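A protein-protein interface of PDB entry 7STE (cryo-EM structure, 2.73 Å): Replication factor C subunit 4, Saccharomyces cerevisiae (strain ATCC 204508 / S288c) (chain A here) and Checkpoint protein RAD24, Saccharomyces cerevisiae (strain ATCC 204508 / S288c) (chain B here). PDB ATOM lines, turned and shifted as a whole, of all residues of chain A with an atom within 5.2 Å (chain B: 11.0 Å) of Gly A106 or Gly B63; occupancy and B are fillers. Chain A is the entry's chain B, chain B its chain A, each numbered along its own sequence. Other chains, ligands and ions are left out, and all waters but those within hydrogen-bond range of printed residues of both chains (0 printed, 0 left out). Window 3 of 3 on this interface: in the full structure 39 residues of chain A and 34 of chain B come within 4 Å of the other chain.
A ring nitrogen (NE2) of His A108 is in hydrogen-bond range of the backbone carbonyl oxygen (O) of Gly B63 (3.0 Å).
The guanidinium group of Arg A139 lies close to the side-chain amide nitrogen of Gln B65, at 3.0 Å.
No residue of chain B comes within 4 Å of Pro A105.
No residue of chain B comes within 4 Å of Lys A107.
Of the printed residues of chain B, His A108 touches Gly B63 (3.0 Å).
Of the printed residues of chain A, Gly B63 touches Gly A106, His A108 and Arg A139.
Of the printed residues of chain A, Gln B65 touches Arg A139.
Of the printed residues of chain A, Thr B323 touches Asn A41.
The nearest residue of chain B that does not touch Gly A106 is Glu B64 (6.1 Å).
The nearest residue of chain A that does not touch Gly B63 is Asn A41 (4.8 Å).
The nearest printed residue of chain A that does not touch Thr B323 is Gly A40 (6.6 Å).
Hydrophobic or aromatic side chains of chain A within 4 Å of the printed part of chain B: His A108.
Among the printed residues, no Asp or Glu carboxylate lies within 4 Å of a Lys or Arg side-chain nitrogen of the other chain.
NE2 of His A108 lies close to O of Gly A106 (3.2 Å).
OE1 of Gln B65 sits at hydrogen-bond distance from OH of Tyr B67.
The side-chain hydroxyl (OG1) of Thr B323 is in hydrogen-bond range of the backbone carbonyl oxygen (O) of Gln B319.
Among the printed residues, pairs that only touch across the chains: Asn A41 with Thr B323 (3.0 Å), Arg A139 with Gly B63 (3.5 Å) and Gly A106 with Gly B63 (3.9 Å).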
ATOM      1  N   GLY A  40       9.434  16.567 -14.889  1.00  0.00           N
ATOM      2  CA  GLY A  40       8.747  16.451 -16.157  1.00  0.00           C
ATOM      3  C   GLY A  40       7.269  16.146 -16.069  1.00  0.00           C
ATOM      4  O   GLY A  40       6.609  16.069 -17.111  1.00  0.00           O
ATOM      5  N   ASN A  41       6.726  15.970 -14.865  1.00  0.00           N
ATOM      6  CA  ASN A  41       5.304  15.715 -14.668  1.00  0.00           C
ATOM      7  C   ASN A  41       4.754  16.772 -13.725  1.00  0.00           C
ATOM      8  O   ASN A  41       5.254  16.932 -12.607  1.00  0.00           O
ATOM      9  CB  ASN A  41       5.067  14.306 -14.117  1.00  0.00           C
ATOM     10  CG  ASN A  41       5.698  13.230 -14.984  1.00  0.00           C
ATOM     11  OD1 ASN A  41       6.230  12.242 -14.479  1.00  0.00           O
ATOM     12  ND2 ASN A  41       5.638  13.416 -16.299  1.00  0.00           N
ATOM     13  N   PRO A 104       5.623  16.223 -27.046  1.00  0.00           N
ATOM     14  CA  PRO A 104       6.383  15.066 -26.564  1.00  0.00           C
ATOM     15  C   PRO A 104       5.667  14.389 -25.411  1.00  0.00           C
ATOM     16  O   PRO A 104       4.875  15.028 -24.700  1.00  0.00           O
ATOM     17  CB  PRO A 104       7.716  15.681 -26.111  1.00  0.00           C
ATOM     18  CG  PRO A 104       7.835  16.936 -26.897  1.00  0.00           C
ATOM     19  CD  PRO A 104       6.433  17.454 -27.015  1.00  0.00           C
ATOM     20  N   PRO A 105       5.912  13.098 -25.191  1.00  0.00           N
ATOM     21  CA  PRO A 105       5.207  12.393 -24.116  1.00  0.00           C
ATOM     22  C   PRO A 105       5.517  12.992 -22.752  1.00  0.00           C
ATOM     23  O   PRO A 105       6.614  13.498 -22.503  1.00  0.00           O
ATOM     24  CB  PRO A 105       5.728  10.957 -24.232  1.00  0.00           C
ATOM     25  CG  PRO A 105       7.068  11.093 -24.865  1.00  0.00           C
ATOM     26  CD  PRO A 105       6.971  12.271 -25.795  1.00  0.00           C
ATOM     27  N   GLY A 106       4.527  12.930 -21.864  1.00  0.00           N
ATOM     28  CA  GLY A 106       4.677  13.447 -20.518  1.00  0.00           C
ATOM     29  C   GLY A 106       4.187  14.872 -20.359  1.00  0.00           C
ATOM     30  O   GLY A 106       3.303  15.139 -19.540  1.00  0.00           O
ATOM     31  N   LYS A 107       4.754  15.796 -21.130  1.00  0.00           N
ATOM     32  CA  LYS A 107       4.367  17.196 -21.015  1.00  0.00           C
ATOM     33  C   LYS A 107       2.904  17.385 -21.399  1.00  0.00           C
ATOM     34  O   LYS A 107       2.392  16.729 -22.311  1.00  0.00           O
ATOM     35  CB  LYS A 107       5.261  18.066 -21.900  1.00  0.00           C
ATOM     36  CG  LYS A 107       6.708  18.134 -21.436  1.00  0.00           C
ATOM     37  CD  LYS A 107       7.508  19.151 -22.234  1.00  0.00           C
ATOM     38  CE  LYS A 107       7.877  18.626 -23.612  1.00  0.00           C
ATOM     39  NZ  LYS A 107       8.847  17.498 -23.538  1.00  0.00           N
ATOM     40  N   HIS A 108       2.232  18.290 -20.691  1.00  0.00           N
ATOM     41  CA  HIS A 108       0.828  18.593 -20.924  1.00  0.00           C
ATOM     42  C   HIS A 108       0.639  20.101 -21.007  1.00  0.00           C
ATOM     43  O   HIS A 108       1.444  20.880 -20.490  1.00  0.00           O
ATOM     44  CB  HIS A 108      -0.066  18.019 -19.815  1.00  0.00           C
ATOM     45  CG  HIS A 108      -0.064  16.523 -19.751  1.00  0.00           C
ATOM     46  ND1 HIS A 108      -0.686  15.736 -20.696  1.00  0.00           N
ATOM     47  CD2 HIS A 108       0.479  15.671 -18.850  1.00  0.00           C
ATOM     48  CE1 HIS A 108      -0.523  14.464 -20.381  1.00  0.00           C
ATOM     49  NE2 HIS A 108       0.180  14.396 -19.266  1.00  0.00           N
ATOM     50  N   ARG A 139      -3.655  20.758 -17.520  1.00  0.00           N
ATOM     51  CA  ARG A 139      -3.507  20.830 -16.073  1.00  0.00           C
ATOM     52  C   ARG A 139      -3.742  22.271 -15.640  1.00  0.00           C
ATOM     53  O   ARG A 139      -3.197  23.200 -16.245  1.00  0.00           O
ATOM     54  CB  ARG A 139      -2.116  20.365 -15.640  1.00  0.00           C
ATOM     55  CG  ARG A 139      -1.810  18.907 -15.951  1.00  0.00           C
ATOM     56  CD  ARG A 139      -2.621  17.929 -15.124  1.00  0.00           C
ATOM     57  NE  ARG A 139      -2.192  16.560 -15.388  1.00  0.00           N
ATOM     58  CZ  ARG A 139      -2.711  15.774 -16.323  1.00  0.00           C
ATOM     59  NH1 ARG A 139      -3.659  16.202 -17.140  1.00  0.00           N
ATOM     60  NH2 ARG A 139      -2.253  14.531 -16.451  1.00  0.00           N
ATOM     61  N   GLY B  63       2.670  10.542 -18.823  1.00  0.00           N
ATOM     62  CA  GLY B  63       1.672  11.593 -18.892  1.00  0.00           C
ATOM     63  C   GLY B  63       0.290  11.110 -18.500  1.00  0.00           C
ATOM     64  O   GLY B  63      -0.480  11.839 -17.874  1.00  0.00           O
ATOM     65  N   GLU B  64      -0.024   9.873 -18.873  1.00  0.00           N
ATOM     66  CA  GLU B  64      -1.327   9.307 -18.557  1.00  0.00           C
ATOM     67  C   GLU B  64      -1.496   9.173 -17.050  1.00  0.00           C
ATOM     68  O   GLU B  64      -0.555   8.837 -16.326  1.00  0.00           O
ATOM     69  CB  GLU B  64      -1.488   7.947 -19.236  1.00  0.00           C
ATOM     70  CG  GLU B  64      -2.886   7.359 -19.140  1.00  0.00           C
ATOM     71  CD  GLU B  64      -3.059   6.137 -20.022  1.00  0.00           C
ATOM     72  OE1 GLU B  64      -2.053   5.673 -20.598  1.00  0.00           O
ATOM     73  OE2 GLU B  64      -4.199   5.641 -20.139  1.00  0.00           O
ATOM     74  N   GLN B  65      -2.710   9.441 -16.579  1.00  0.00           N
ATOM     75  CA  GLN B  65      -3.015   9.430 -15.158  1.00  0.00           C
ATOM     76  C   GLN B  65      -3.341   8.023 -14.673  1.00  0.00           C
ATOM     77  O   GLN B  65      -3.864   7.190 -15.419  1.00  0.00           O
ATOM     78  CB  GLN B  65      -4.180  10.373 -14.864  1.00  0.00           C
ATOM     79  CG  GLN B  65      -3.824  11.839 -15.030  1.00  0.00           C
ATOM     80  CD  GLN B  65      -5.035  12.739 -14.971  1.00  0.00           C
ATOM     81  OE1 GLN B  65      -6.171  12.270 -14.975  1.00  0.00           O
ATOM     82  NE2 GLN B  65      -4.798  14.039 -14.870  1.00  0.00           N
ATOM     83  N   TRP B  66      -3.021   7.768 -13.404  1.00  0.00           N
ATOM     84  CA  TRP B  66      -3.160   6.424 -12.850  1.00  0.00           C
ATOM     85  C   TRP B  66      -4.625   6.023 -12.713  1.00  0.00           C
ATOM     86  O   TRP B  66      -5.018   4.929 -13.132  1.00  0.00           O
ATOM     87  CB  TRP B  66      -2.455   6.348 -11.496  1.00  0.00           C
ATOM     88  CG  TRP B  66      -0.993   6.013 -11.580  1.00  0.00           C
ATOM     89  CD1 TRP B  66      -0.192   6.081 -12.684  1.00  0.00           C
ATOM     90  CD2 TRP B  66      -0.154   5.576 -10.504  1.00  0.00           C
ATOM     91  NE1 TRP B  66       1.090   5.702 -12.364  1.00  0.00           N
ATOM     92  CE2 TRP B  66       1.139   5.388 -11.031  1.00  0.00           C
ATOM     93  CE3 TRP B  66      -0.373   5.322  -9.147  1.00  0.00           C
ATOM     94  CZ2 TRP B  66       2.208   4.958 -10.249  1.00  0.00           C
ATOM     95  CZ3 TRP B  66       0.690   4.894  -8.373  1.00  0.00           C
ATOM     96  CH2 TRP B  66       1.963   4.717  -8.925  1.00  0.00           C
ATOM     97  N   TYR B  67      -5.451   6.895 -12.128  1.00  0.00           N
ATOM     98  CA  TYR B  67      -6.829   6.506 -11.842  1.00  0.00           C
ATOM     99  C   TYR B  67      -7.592   6.207 -13.126  1.00  0.00           C
ATOM    100  O   TYR B  67      -8.428   5.296 -13.162  1.00  0.00           O
ATOM    101  CB  TYR B  67      -7.536   7.593 -11.028  1.00  0.00           C
ATOM    102  CG  TYR B  67      -7.717   8.911 -11.742  1.00  0.00           C
ATOM    103  CD1 TYR B  67      -6.714   9.871 -11.740  1.00  0.00           C
ATOM    104  CD2 TYR B  67      -8.903   9.204 -12.402  1.00  0.00           C
ATOM    105  CE1 TYR B  67      -6.883  11.079 -12.386  1.00  0.00           C
ATOM    106  CE2 TYR B  67      -9.081  10.409 -13.051  1.00  0.00           C
ATOM    107  CZ  TYR B  67      -8.069  11.344 -13.038  1.00  0.00           C
ATOM    108  OH  TYR B  67      -8.244  12.545 -13.685  1.00  0.00           O
ATOM    109  N   GLU B  68      -7.320   6.962 -14.192  1.00  0.00           N
ATOM    110  CA  GLU B  68      -7.913   6.639 -15.485  1.00  0.00           C
ATOM    111  C   GLU B  68      -7.448   5.271 -15.970  1.00  0.00           C
ATOM    112  O   GLU B  68      -8.239   4.495 -16.518  1.00  0.00           O
ATOM    113  CB  GLU B  68      -7.561   7.719 -16.509  1.00  0.00           C
ATOM    114  CG  GLU B  68      -8.453   7.715 -17.745  1.00  0.00           C
ATOM    115  CD  GLU B  68      -8.588   9.085 -18.387  1.00  0.00           C
ATOM    116  OE1 GLU B  68      -8.148  10.083 -17.779  1.00  0.00           O
ATOM    117  OE2 GLU B  68      -9.136   9.163 -19.506  1.00  0.00           O
ATOM    118  N   LYS B  69      -6.164   4.960 -15.779  1.00  0.00           N
ATOM    119  CA  LYS B  69      -5.647   3.660 -16.192  1.00  0.00           C
ATOM    120  C   LYS B  69      -6.319   2.526 -15.429  1.00  0.00           C
ATOM    121  O   LYS B  69      -6.686   1.503 -16.017  1.00  0.00           O
ATOM    122  CB  LYS B  69      -4.133   3.605 -15.981  1.00  0.00           C
ATOM    123  CG  LYS B  69      -3.316   4.278 -17.067  1.00  0.00           C
ATOM    124  CD  LYS B  69      -1.853   3.869 -16.973  1.00  0.00           C
ATOM    125  CE  LYS B  69      -0.931   4.939 -17.528  1.00  0.00           C
ATOM    126  NZ  LYS B  69       0.496   4.674 -17.195  1.00  0.00           N
ATOM    127  N   MET B 287       7.631  -0.385 -11.305  1.00  0.00           N
ATOM    128  CA  MET B 287       8.256   0.930 -11.212  1.00  0.00           C
ATOM    129  C   MET B 287       8.640   1.258  -9.775  1.00  0.00           C
ATOM    130  O   MET B 287       9.637   1.951  -9.538  1.00  0.00           O
ATOM    131  CB  MET B 287       7.320   1.997 -11.783  1.00  0.00           C
ATOM    132  CG  MET B 287       6.029   2.185 -11.006  1.00  0.00           C
ATOM    133  SD  MET B 287       4.981   3.466 -11.719  1.00  0.00           S
ATOM    134  CE  MET B 287       5.896   4.941 -11.278  1.00  0.00           C
ATOM    135  N   LYS B 291      12.393   2.311  -8.730  1.00  0.00           N
ATOM    136  CA  LYS B 291      12.725   3.495  -7.947  1.00  0.00           C
ATOM    137  C   LYS B 291      13.087   3.171  -6.503  1.00  0.00           C
ATOM    138  O   LYS B 291      13.529   4.068  -5.777  1.00  0.00           O
ATOM    139  CB  LYS B 291      11.553   4.480  -7.970  1.00  0.00           C
ATOM    140  CG  LYS B 291      11.171   4.948  -9.364  1.00  0.00           C
ATOM    141  CD  LYS B 291      10.716   6.398  -9.361  1.00  0.00           C
ATOM    142  CE  LYS B 291      10.082   6.783 -10.687  1.00  0.00           C
ATOM    143  NZ  LYS B 291       8.606   6.592 -10.678  1.00  0.00           N
ATOM    144  N   THR B 316      -4.251  10.484  -7.179  1.00  0.00           N
ATOM    145  CA  THR B 316      -3.373  11.503  -7.743  1.00  0.00           C
ATOM    146  C   THR B 316      -2.196  11.787  -6.817  1.00  0.00           C
ATOM    147  O   THR B 316      -1.055  11.921  -7.273  1.00  0.00           O
ATOM    148  CB  THR B 316      -4.162  12.786  -8.013  1.00  0.00           C
ATOM    149  OG1 THR B 316      -5.270  12.498  -8.875  1.00  0.00           O
ATOM    150  CG2 THR B 316      -3.273  13.836  -8.669  1.00  0.00           C
ATOM    151  N   GLN B 319       0.254   8.893  -7.037  1.00  0.00           N
ATOM    152  CA  GLN B 319       1.032   8.966  -8.270  1.00  0.00           C
ATOM    153  C   GLN B 319       2.091  10.056  -8.184  1.00  0.00           C
ATOM    154  O   GLN B 319       3.233   9.859  -8.616  1.00  0.00           O
ATOM    155  CB  GLN B 319       0.104   9.211  -9.460  1.00  0.00           C
ATOM    156  CG  GLN B 319       0.823   9.297 -10.799  1.00  0.00           C
ATOM    157  CD  GLN B 319      -0.135   9.395 -11.970  1.00  0.00           C
ATOM    158  OE1 GLN B 319      -1.316   9.696 -11.798  1.00  0.00           O
ATOM    159  NE2 GLN B 319       0.372   9.141 -13.172  1.00  0.00           N
ATOM    160  N   PHE B 320       1.732  11.216  -7.631  1.00  0.00           N
ATOM    161  CA  PHE B 320       2.700  12.300  -7.494  1.00  0.00           C
ATOM    162  C   PHE B 320       3.851  11.894  -6.582  1.00  0.00           C
ATOM    163  O   PHE B 320       5.018  12.170  -6.883  1.00  0.00           O
ATOM    164  CB  PHE B 320       2.007  13.553  -6.960  1.00  0.00           C
ATOM    165  CG  PHE B 320       2.940  14.707  -6.720  1.00  0.00           C
ATOM    166  CD1 PHE B 320       3.937  15.014  -7.631  1.00  0.00           C
ATOM    167  CD2 PHE B 320       2.817  15.487  -5.582  1.00  0.00           C
ATOM    168  CE1 PHE B 320       4.795  16.074  -7.411  1.00  0.00           C
ATOM    169  CE2 PHE B 320       3.672  16.549  -5.357  1.00  0.00           C
ATOM    170  CZ  PHE B 320       4.662  16.842  -6.272  1.00  0.00           C
ATOM    171  N   THR B 323       6.090   9.432  -8.429  1.00  0.00           N
ATOM    172  CA  THR B 323       6.855  10.102  -9.473  1.00  0.00           C
ATOM    173  C   THR B 323       7.924  11.027  -8.905  1.00  0.00           C
ATOM    174  O   THR B 323       9.056  11.043  -9.402  1.00  0.00           O
ATOM    175  CB  THR B 323       5.914  10.902 -10.379  1.00  0.00           C
ATOM    176  OG1 THR B 323       4.779  10.098 -10.727  1.00  0.00           O
ATOM    177  CG2 THR B 323       6.629  11.339 -11.645  1.00  0.00           C
